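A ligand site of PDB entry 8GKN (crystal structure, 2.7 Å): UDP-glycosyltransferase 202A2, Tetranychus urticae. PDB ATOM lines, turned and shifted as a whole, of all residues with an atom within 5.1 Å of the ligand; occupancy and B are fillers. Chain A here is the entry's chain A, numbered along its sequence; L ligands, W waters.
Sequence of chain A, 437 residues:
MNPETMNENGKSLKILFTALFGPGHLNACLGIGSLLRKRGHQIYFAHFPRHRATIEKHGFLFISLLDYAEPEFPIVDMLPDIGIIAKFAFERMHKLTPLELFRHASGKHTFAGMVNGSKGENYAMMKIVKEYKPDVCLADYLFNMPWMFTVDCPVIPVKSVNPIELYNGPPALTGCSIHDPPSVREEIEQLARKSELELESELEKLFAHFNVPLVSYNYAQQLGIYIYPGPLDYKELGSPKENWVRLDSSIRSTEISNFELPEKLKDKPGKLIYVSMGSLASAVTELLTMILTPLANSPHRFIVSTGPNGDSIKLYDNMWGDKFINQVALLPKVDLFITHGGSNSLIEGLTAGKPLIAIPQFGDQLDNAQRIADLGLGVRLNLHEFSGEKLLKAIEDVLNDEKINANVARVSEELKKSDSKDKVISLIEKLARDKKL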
ATOM      1  N   PRO A  23       2.571   5.038 -14.455  1.00  0.00           N
ATOM      2  CA  PRO A  23       1.352   5.780 -14.129  1.00  0.00           C
ATOM      3  C   PRO A  23       0.344   4.995 -13.296  1.00  0.00           C
ATOM      4  O   PRO A  23      -0.363   5.582 -12.489  1.00  0.00           O
ATOM      5  CB  PRO A  23       0.761   6.135 -15.499  1.00  0.00           C
ATOM      6  CG  PRO A  23       1.994   6.310 -16.352  1.00  0.00           C
ATOM      7  CD  PRO A  23       2.963   5.255 -15.867  1.00  0.00           C
ATOM      8  N   GLY A  24       0.295   3.679 -13.480  1.00  0.00           N
ATOM      9  CA  GLY A  24      -0.646   2.832 -12.728  1.00  0.00           C
ATOM     10  C   GLY A  24      -0.357   2.805 -11.248  1.00  0.00           C
ATOM     11  O   GLY A  24      -1.302   2.927 -10.454  1.00  0.00           O
ATOM     12  N   ASN A  27      -1.211   6.106  -9.787  1.00  0.00           N
ATOM     13  CA  ASN A  27      -2.624   6.423  -9.751  1.00  0.00           C
ATOM     14  C   ASN A  27      -3.243   5.815  -8.496  1.00  0.00           C
ATOM     15  O   ASN A  27      -4.095   6.416  -7.854  1.00  0.00           O
ATOM     16  CB  ASN A  27      -3.357   5.977 -11.019  1.00  0.00           C
ATOM     17  CG  ASN A  27      -3.140   6.912 -12.212  1.00  0.00           C
ATOM     18  OD1 ASN A  27      -2.736   8.067 -12.057  1.00  0.00           O
ATOM     19  ND2 ASN A  27      -3.398   6.427 -13.424  1.00  0.00           N
ATOM     20  N   ARG A 252      -8.621   7.818  -8.333  1.00  0.00           N
ATOM     21  CA  ARG A 252      -8.588   9.291  -8.174  1.00  0.00           C
ATOM     22  C   ARG A 252      -9.877   9.869  -8.750  1.00  0.00           C
ATOM     23  O   ARG A 252     -10.472   9.225  -9.633  1.00  0.00           O
ATOM     24  CB  ARG A 252      -7.382   9.812  -8.945  1.00  0.00           C
ATOM     25  CG  ARG A 252      -7.422   9.482 -10.428  1.00  0.00           C
ATOM     26  CD  ARG A 252      -6.067   9.290 -11.068  1.00  0.00           C
ATOM     27  NE  ARG A 252      -6.156   8.844 -12.453  1.00  0.00           N
ATOM     28  CZ  ARG A 252      -6.700   7.686 -12.843  1.00  0.00           C
ATOM     29  NH1 ARG A 252      -6.793   7.410 -14.135  1.00  0.00           N
ATOM     30  NH2 ARG A 252      -7.143   6.823 -11.955  1.00  0.00           N
ATOM     31  N   TYR A 274     -14.513   0.572 -25.546  1.00  0.00           N
ATOM     32  CA  TYR A 274     -13.262   1.248 -25.280  1.00  0.00           C
ATOM     33  C   TYR A 274     -12.098   0.269 -25.430  1.00  0.00           C
ATOM     34  O   TYR A 274     -12.232  -0.866 -25.002  1.00  0.00           O
ATOM     35  CB  TYR A 274     -13.300   1.848 -23.885  1.00  0.00           C
ATOM     36  CG  TYR A 274     -12.023   2.471 -23.400  1.00  0.00           C
ATOM     37  CD1 TYR A 274     -11.315   3.356 -24.189  1.00  0.00           C
ATOM     38  CD2 TYR A 274     -11.555   2.257 -22.113  1.00  0.00           C
ATOM     39  CE1 TYR A 274     -10.158   3.965 -23.758  1.00  0.00           C
ATOM     40  CE2 TYR A 274     -10.384   2.860 -21.662  1.00  0.00           C
ATOM     41  CZ  TYR A 274      -9.695   3.716 -22.490  1.00  0.00           C
ATOM     42  OH  TYR A 274      -8.569   4.369 -22.063  1.00  0.00           O
ATOM     43  N   SER A 276      -7.863  -0.076 -24.638  1.00  0.00           N
ATOM     44  CA  SER A 276      -6.626   0.462 -24.086  1.00  0.00           C
ATOM     45  C   SER A 276      -5.727  -0.667 -23.656  1.00  0.00           C
ATOM     46  O   SER A 276      -6.196  -1.548 -22.925  1.00  0.00           O
ATOM     47  CB  SER A 276      -6.833   1.368 -22.900  1.00  0.00           C
ATOM     48  OG  SER A 276      -5.581   1.829 -22.394  1.00  0.00           O
ATOM     49  N   MET A 277      -4.452  -0.575 -24.043  1.00  0.00           N
ATOM     50  CA  MET A 277      -3.444  -1.554 -23.668  1.00  0.00           C
ATOM     51  C   MET A 277      -2.559  -0.953 -22.577  1.00  0.00           C
ATOM     52  O   MET A 277      -1.510  -1.502 -22.257  1.00  0.00           O
ATOM     53  CB  MET A 277      -2.614  -1.953 -24.896  1.00  0.00           C
ATOM     54  CG  MET A 277      -3.376  -2.821 -25.875  1.00  0.00           C
ATOM     55  SD  MET A 277      -3.977  -4.404 -25.202  1.00  0.00           S
ATOM     56  CE  MET A 277      -5.748  -4.189 -25.314  1.00  0.00           C
ATOM     57  N   GLY A 278      -3.023   0.151 -21.993  1.00  0.00           N
ATOM     58  CA  GLY A 278      -2.458   0.701 -20.767  1.00  0.00           C
ATOM     59  C   GLY A 278      -1.484   1.840 -21.021  1.00  0.00           C
ATOM     60  O   GLY A 278      -1.337   2.281 -22.143  1.00  0.00           O
ATOM     61  N   SER A 279      -0.795   2.281 -19.970  1.00  0.00           N
ATOM     62  CA  SER A 279       0.228   3.314 -20.090  1.00  0.00           C
ATOM     63  C   SER A 279       1.565   2.779 -20.610  1.00  0.00           C
ATOM     64  O   SER A 279       2.363   3.577 -21.082  1.00  0.00           O
ATOM     65  CB  SER A 279       0.414   4.024 -18.748  1.00  0.00           C
ATOM     66  OG  SER A 279       0.685   3.124 -17.679  1.00  0.00           O
ATOM     67  N   LEU A 280       1.842   1.472 -20.553  1.00  0.00           N
ATOM     68  CA  LEU A 280       3.192   0.978 -20.812  1.00  0.00           C
ATOM     69  C   LEU A 280       3.258   0.210 -22.137  1.00  0.00           C
ATOM     70  O   LEU A 280       4.020   0.623 -23.015  1.00  0.00           O
ATOM     71  CB  LEU A 280       3.687   0.132 -19.647  1.00  0.00           C
ATOM     72  CG  LEU A 280       3.873   0.868 -18.321  1.00  0.00           C
ATOM     73  CD1 LEU A 280       4.580  -0.005 -17.300  1.00  0.00           C
ATOM     74  CD2 LEU A 280       4.680   2.151 -18.457  1.00  0.00           C
ATOM     75  N   SER A 305      -7.471   4.437 -26.767  1.00  0.00           N
ATOM     76  CA  SER A 305      -6.242   5.041 -26.298  1.00  0.00           C
ATOM     77  C   SER A 305      -5.081   4.548 -27.165  1.00  0.00           C
ATOM     78  O   SER A 305      -4.801   3.350 -27.204  1.00  0.00           O
ATOM     79  CB  SER A 305      -6.064   4.720 -24.889  1.00  0.00           C
ATOM     80  OG  SER A 305      -4.879   5.337 -24.448  1.00  0.00           O
ATOM     81  N   LYS A 323      -3.881   9.888 -27.906  1.00  0.00           N
ATOM     82  CA  LYS A 323      -2.773   9.260 -27.209  1.00  0.00           C
ATOM     83  C   LYS A 323      -3.173   8.924 -25.773  1.00  0.00           C
ATOM     84  O   LYS A 323      -2.838   7.858 -25.273  1.00  0.00           O
ATOM     85  CB  LYS A 323      -1.556  10.184 -27.297  1.00  0.00           C
ATOM     86  CG  LYS A 323      -1.086  10.465 -28.717  1.00  0.00           C
ATOM     87  CD  LYS A 323       0.336  10.949 -28.848  1.00  0.00           C
ATOM     88  CE  LYS A 323       0.722  11.936 -27.769  1.00  0.00           C
ATOM     89  NZ  LYS A 323       1.850  12.772 -28.205  1.00  0.00           N
ATOM     90  N   PHE A 324      -3.915   9.840 -25.144  1.00  0.00           N
ATOM     91  CA  PHE A 324      -4.402   9.721 -23.773  1.00  0.00           C
ATOM     92  C   PHE A 324      -5.888  10.094 -23.716  1.00  0.00           C
ATOM     93  O   PHE A 324      -6.307  11.065 -24.342  1.00  0.00           O
ATOM     94  CB  PHE A 324      -3.573  10.647 -22.878  1.00  0.00           C
ATOM     95  CG  PHE A 324      -3.720  10.423 -21.406  1.00  0.00           C
ATOM     96  CD1 PHE A 324      -3.236   9.265 -20.796  1.00  0.00           C
ATOM     97  CD2 PHE A 324      -4.397  11.371 -20.624  1.00  0.00           C
ATOM     98  CE1 PHE A 324      -3.391   9.073 -19.434  1.00  0.00           C
ATOM     99  CE2 PHE A 324      -4.557  11.175 -19.255  1.00  0.00           C
ATOM    100  CZ  PHE A 324      -4.057  10.027 -18.668  1.00  0.00           C
ATOM    101  N   ILE A 325      -6.654   9.287 -22.963  1.00  0.00           N
ATOM    102  CA  ILE A 325      -8.122   9.469 -22.853  1.00  0.00           C
ATOM    103  C   ILE A 325      -8.500   9.606 -21.377  1.00  0.00           C
ATOM    104  O   ILE A 325      -7.740   9.116 -20.551  1.00  0.00           O
ATOM    105  CB  ILE A 325      -8.814   8.234 -23.463  1.00  0.00           C
ATOM    106  CG1 ILE A 325      -8.397   7.985 -24.917  1.00  0.00           C
ATOM    107  CG2 ILE A 325     -10.327   8.320 -23.321  1.00  0.00           C
ATOM    108  CD1 ILE A 325      -9.144   8.828 -25.927  1.00  0.00           C
ATOM    109  N   ASN A 326      -9.623  10.255 -21.070  1.00  0.00           N
ATOM    110  CA  ASN A 326     -10.135  10.274 -19.675  1.00  0.00           C
ATOM    111  C   ASN A 326     -10.917   8.977 -19.500  1.00  0.00           C
ATOM    112  O   ASN A 326     -12.087   8.948 -19.873  1.00  0.00           O
ATOM    113  CB  ASN A 326     -10.946  11.523 -19.351  1.00  0.00           C
ATOM    114  CG  ASN A 326     -11.177  11.706 -17.864  1.00  0.00           C
ATOM    115  OD1 ASN A 326     -10.757  10.892 -17.056  1.00  0.00           O
ATOM    116  ND2 ASN A 326     -11.847  12.782 -17.496  1.00  0.00           N
ATOM    117  N   GLN A 327     -10.257   7.940 -18.999  1.00  0.00           N
ATOM    118  CA  GLN A 327     -10.857   6.596 -18.868  1.00  0.00           C
ATOM    119  C   GLN A 327     -11.953   6.578 -17.810  1.00  0.00           C
ATOM    120  O   GLN A 327     -12.971   5.927 -18.053  1.00  0.00           O
ATOM    121  CB  GLN A 327      -9.704   5.631 -18.563  1.00  0.00           C
ATOM    122  CG  GLN A 327     -10.100   4.173 -18.525  1.00  0.00           C
ATOM    123  CD  GLN A 327      -8.869   3.299 -18.427  1.00  0.00           C
ATOM    124  OE1 GLN A 327      -7.988   3.339 -19.280  1.00  0.00           O
ATOM    125  NE2 GLN A 327      -8.801   2.509 -17.370  1.00  0.00           N
ATOM    126  N   VAL A 328     -11.765   7.278 -16.706  1.00  0.00           N
ATOM    127  CA  VAL A 328     -12.751   7.226 -15.595  1.00  0.00           C
ATOM    128  C   VAL A 328     -14.023   7.958 -16.030  1.00  0.00           C
ATOM    129  O   VAL A 328     -15.106   7.513 -15.635  1.00  0.00           O
ATOM    130  CB  VAL A 328     -12.166   7.793 -14.295  1.00  0.00           C
ATOM    131  CG1 VAL A 328     -13.188   7.856 -13.176  1.00  0.00           C
ATOM    132  CG2 VAL A 328     -10.937   7.023 -13.854  1.00  0.00           C
ATOM    133  N   HIS A 340      -5.737  -4.571 -21.350  1.00  0.00           N
ATOM    134  CA  HIS A 340      -4.573  -5.432 -21.230  1.00  0.00           C
ATOM    135  C   HIS A 340      -4.563  -6.222 -19.941  1.00  0.00           C
ATOM    136  O   HIS A 340      -3.679  -7.038 -19.734  1.00  0.00           O
ATOM    137  CB  HIS A 340      -3.269  -4.630 -21.239  1.00  0.00           C
ATOM    138  CG  HIS A 340      -3.097  -3.665 -20.129  1.00  0.00           C
ATOM    139  ND1 HIS A 340      -4.089  -2.785 -19.750  1.00  0.00           N
ATOM    140  CD2 HIS A 340      -2.054  -3.412 -19.340  1.00  0.00           C
ATOM    141  CE1 HIS A 340      -3.647  -2.021 -18.759  1.00  0.00           C
ATOM    142  NE2 HIS A 340      -2.405  -2.379 -18.493  1.00  0.00           N
ATOM    143  N   GLY A 342      -4.457  -4.703 -16.890  1.00  0.00           N
ATOM    144  CA  GLY A 342      -3.889  -3.940 -15.794  1.00  0.00           C
ATOM    145  C   GLY A 342      -4.899  -3.779 -14.654  1.00  0.00           C
ATOM    146  O   GLY A 342      -6.103  -3.728 -14.900  1.00  0.00           O
ATOM    147  N   SER A 343      -4.386  -3.676 -13.413  1.00  0.00           N
ATOM    148  CA  SER A 343      -5.217  -3.676 -12.233  1.00  0.00           C
ATOM    149  C   SER A 343      -6.122  -2.456 -12.172  1.00  0.00           C
ATOM    150  O   SER A 343      -7.298  -2.599 -11.865  1.00  0.00           O
ATOM    151  CB  SER A 343      -4.410  -3.823 -10.971  1.00  0.00           C
ATOM    152  OG  SER A 343      -4.097  -5.205 -10.761  1.00  0.00           O
ATOM    153  N   ASN A 344      -5.570  -1.267 -12.403  1.00  0.00           N
ATOM    154  CA  ASN A 344      -6.346  -0.031 -12.280  1.00  0.00           C
ATOM    155  C   ASN A 344      -7.462  -0.010 -13.311  1.00  0.00           C
ATOM    156  O   ASN A 344      -8.570   0.462 -13.040  1.00  0.00           O
ATOM    157  CB  ASN A 344      -5.493   1.214 -12.463  1.00  0.00           C
ATOM    158  CG  ASN A 344      -4.550   1.454 -11.309  1.00  0.00           C
ATOM    159  OD1 ASN A 344      -4.917   2.073 -10.318  1.00  0.00           O
ATOM    160  ND2 ASN A 344      -3.333   0.968 -11.427  1.00  0.00           N
ATOM    161  N   SER A 345      -7.159  -0.514 -14.510  1.00  0.00           N
ATOM    162  CA  SER A 345      -8.143  -0.543 -15.569  1.00  0.00           C
ATOM    163  C   SER A 345      -9.227  -1.550 -15.197  1.00  0.00           C
ATOM    164  O   SER A 345     -10.400  -1.326 -15.428  1.00  0.00           O
ATOM    165  CB  SER A 345      -7.485  -0.837 -16.892  1.00  0.00           C
ATOM    166  OG  SER A 345      -6.648   0.236 -17.314  1.00  0.00           O
ATOM    167  N   LEU A 346      -8.820  -2.663 -14.638  1.00  0.00           N
ATOM    168  CA  LEU A 346      -9.727  -3.697 -14.172  1.00  0.00           C
ATOM    169  C   LEU A 346     -10.719  -3.119 -13.147  1.00  0.00           C
ATOM    170  O   LEU A 346     -11.944  -3.369 -13.220  1.00  0.00           O
ATOM    171  CB  LEU A 346      -8.850  -4.807 -13.594  1.00  0.00           C
ATOM    172  CG  LEU A 346      -9.545  -5.894 -12.787  1.00  0.00           C
ATOM    173  CD1 LEU A 346     -10.465  -6.724 -13.671  1.00  0.00           C
ATOM    174  CD2 LEU A 346      -8.515  -6.772 -12.133  1.00  0.00           C
ATOM    175  N   GLU A 348     -11.372   0.195 -12.381  1.00  0.00           N
ATOM    176  CA  GLU A 348     -12.196   1.253 -12.955  1.00  0.00           C
ATOM    177  C   GLU A 348     -13.295   0.650 -13.825  1.00  0.00           C
ATOM    178  O   GLU A 348     -14.442   1.086 -13.806  1.00  0.00           O
ATOM    179  CB  GLU A 348     -11.354   2.237 -13.762  1.00  0.00           C
ATOM    180  CG  GLU A 348     -10.383   3.045 -12.915  1.00  0.00           C
ATOM    181  CD  GLU A 348      -9.098   3.487 -13.608  1.00  0.00           C
ATOM    182  OE1 GLU A 348      -9.013   3.418 -14.893  1.00  0.00           O
ATOM    183  OE2 GLU A 348      -8.181   3.907 -12.881  1.00  0.00           O
ATOM    184  N   PHE A 362       1.976  -8.453 -19.948  1.00  0.00           N
ATOM    185  CA  PHE A 362       3.116  -8.768 -19.086  1.00  0.00           C
ATOM    186  C   PHE A 362       2.737  -8.827 -17.612  1.00  0.00           C
ATOM    187  O   PHE A 362       1.706  -8.342 -17.189  1.00  0.00           O
ATOM    188  CB  PHE A 362       4.218  -7.709 -19.254  1.00  0.00           C
ATOM    189  CG  PHE A 362       3.837  -6.291 -18.899  1.00  0.00           C
ATOM    190  CD1 PHE A 362       3.174  -5.469 -19.804  1.00  0.00           C
ATOM    191  CD2 PHE A 362       4.143  -5.773 -17.652  1.00  0.00           C
ATOM    192  CE1 PHE A 362       2.859  -4.142 -19.489  1.00  0.00           C
ATOM    193  CE2 PHE A 362       3.818  -4.453 -17.322  1.00  0.00           C
ATOM    194  CZ  PHE A 362       3.171  -3.638 -18.245  1.00  0.00           C
ATOM    195  N   GLN A 365      -0.747  -8.961 -15.269  1.00  0.00           N
ATOM    196  CA  GLN A 365      -1.867  -8.952 -16.190  1.00  0.00           C
ATOM    197  C   GLN A 365      -2.335 -10.367 -16.527  1.00  0.00           C
ATOM    198  O   GLN A 365      -3.517 -10.596 -16.728  1.00  0.00           O
ATOM    199  CB  GLN A 365      -1.490  -8.222 -17.468  1.00  0.00           C
ATOM    200  CG  GLN A 365      -1.306  -6.738 -17.272  1.00  0.00           C
ATOM    201  CD  GLN A 365      -0.414  -6.172 -18.346  1.00  0.00           C
ATOM    202  OE1 GLN A 365      -0.413  -6.610 -19.491  1.00  0.00           O
ATOM    203  NE2 GLN A 365       0.425  -5.230 -17.945  1.00  0.00           N
HETATM  204  N1  LIG L   1      -5.064   5.683 -18.396  1.00  0.00           N
HETATM  205  C1  LIG L   1      -5.771   6.826 -18.692  1.00  0.00           C
HETATM  206  N2  LIG L   1      -5.909   7.080 -20.034  1.00  0.00           N
HETATM  207  C2  LIG L   1      -5.436   6.325 -21.081  1.00  0.00           C
HETATM  208  C3  LIG L   1      -4.719   5.144 -20.688  1.00  0.00           C
HETATM  209  C4  LIG L   1      -4.566   4.872 -19.383  1.00  0.00           C
HETATM  210  O1  LIG L   1      -6.221   7.571 -17.841  1.00  0.00           O
HETATM  211  O2  LIG L   1      -5.650   6.687 -22.238  1.00  0.00           O
HETATM  212  C5  LIG L   1      -4.873   5.355 -16.968  1.00  0.00           C
HETATM  213  C6  LIG L   1      -5.937   4.422 -16.420  1.00  0.00           C
HETATM  214  O3  LIG L   1      -7.044   5.187 -15.976  1.00  0.00           O
HETATM  215  C7  LIG L   1      -5.191   3.727 -15.270  1.00  0.00           C
HETATM  216  C8  LIG L   1      -3.743   3.678 -15.784  1.00  0.00           C
HETATM  217  O4  LIG L   1      -3.642   4.685 -16.825  1.00  0.00           O
HETATM  218  O5  LIG L   1      -5.269   4.482 -14.064  1.00  0.00           O
HETATM  219  C9  LIG L   1      -3.293   2.335 -16.320  1.00  0.00           C
HETATM  220  O6  LIG L   1      -2.971   1.474 -15.210  1.00  0.00           O
HETATM  221  P1  LIG L   1      -3.190  -0.108 -15.342  1.00  0.00           P
HETATM  222  O7  LIG L   1      -4.522  -0.365 -15.952  1.00  0.00           O
HETATM  223  O8  LIG L   1      -2.874  -0.758 -14.032  1.00  0.00           O
HETATM  224  O9  LIG L   1      -2.063  -0.509 -16.404  1.00  0.00           O
HETATM  225  P2  LIG L   1      -0.452  -0.366 -16.433  1.00  0.00           P
HETATM  226  O10 LIG L   1       0.005  -1.204 -17.591  1.00  0.00           O
HETATM  227  O11 LIG L   1       0.023  -0.884 -15.110  1.00  0.00           O
HETATM  228  O12 LIG L   1      -0.161   1.094 -16.626  1.00  0.00           O
HETATM  229  O   HOH W   1      -5.791   1.796 -19.780  1.00  0.00           O
HETATM  230  O   HOH W   2       0.538  -1.228 -20.070  1.00  0.00           O
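Residues that only touch the ligand: Gly 24, Tyr 274, Ser 276, Phe 324 and Gly 342. Hydrophobic or aromatic side chains that line the ligand: Phe 324, Ile 325 and His 340.
ND2 of Asn 344 is in hydrogen-bond range of O8 of the ligand (3.2 Å). O3 of the ligand sits at hydrogen-bond distance from OE1 of Glu 348 (2.9 Å). The backbone NH (N) of Asn 344 is in hydrogen-bond range of an oxygen (O8) of the ligand (3.2 Å). The backbone NH (N) of Ser 345 is in hydrogen-bond range of an oxygen (O7) of the ligand, 3.0 Å away. O5 of the ligand sits at hydrogen-bond distance from ND2 of Asn 27 (2.8 Å). An oxygen (O7) of the ligand sits at hydrogen-bond distance from the side-chain hydroxyl of Ser 345 (2.6 Å). The backbone carbonyl oxygen (O) of Ile 325 is in hydrogen-bond range of a nitrogen (N2) of the ligand, 2.8 Å away. The guanidinium group (NH1) of Arg 252 lies within hydrogen-bond range of an oxygen (O3) of the ligand. O2 of the ligand is in hydrogen-bond range of OG of Ser 305, at 2.7 Å. The backbone NH (N) of Ile 325 lies within hydrogen-bond range of an oxygen (O2) of the ligand (2.9 Å). An oxygen (O3) of the ligand is in hydrogen-bond range of the side-chain amide nitrogen (NE2) of Gln 327 (3.5 Å). An oxygen (O9) of the ligand sits at hydrogen-bond distance from a ring nitrogen (NE2) of His 340 (2.8 Å). An oxygen (O12) of the ligand is in hydrogen-bond range of the side-chain hydroxyl (OG) of Ser 279 (2.4 Å). The backbone NH (N) of Ser 343 sits at hydrogen-bond distance from an oxygen (O8) of the ligand.
Water W2 lies within hydrogen-bond range of O10 of the ligand (2.5 Å), O of Met 277 (3.0 Å) and N of Leu 280 (3.0 Å). Water W1 lies within hydrogen-bond range of the side-chain hydroxyl (OG) of Ser 276, the side-chain amide oxygen (OE1) of Gln 327 and the side-chain hydroxyl (OG) of Ser 345.
The side-chain hydroxyl (OG) of Ser 305 sits at hydrogen-bond distance from the backbone carbonyl oxygen (O) of Lys 323 (3.3 Å). ND2 of Asn 344 is in hydrogen-bond range of O of Gly 24 (3.0 Å). The guanidinium group of Arg 252 lies within salt-bridge range of the side-chain carboxylate of Glu 348 (3.2 Å). The side-chain carboxylate (OE1) of Glu 348 sits at hydrogen-bond distance from the side-chain amide nitrogen (NE2) of Gln 327. ND1 of His 340 lies close to N of Gly 342, at 3.5 Å. OE1 of Gln 327 sits at hydrogen-bond distance from OH of Tyr 274, at 3.0 Å. ND2 of Asn 27 sits close to O of Pro 23 (3.3 Å). The side-chain hydroxyl (OG) of Ser 345 is in hydrogen-bond range of the side-chain amide nitrogen (NE2) of Gln 327 (3.1 Å).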
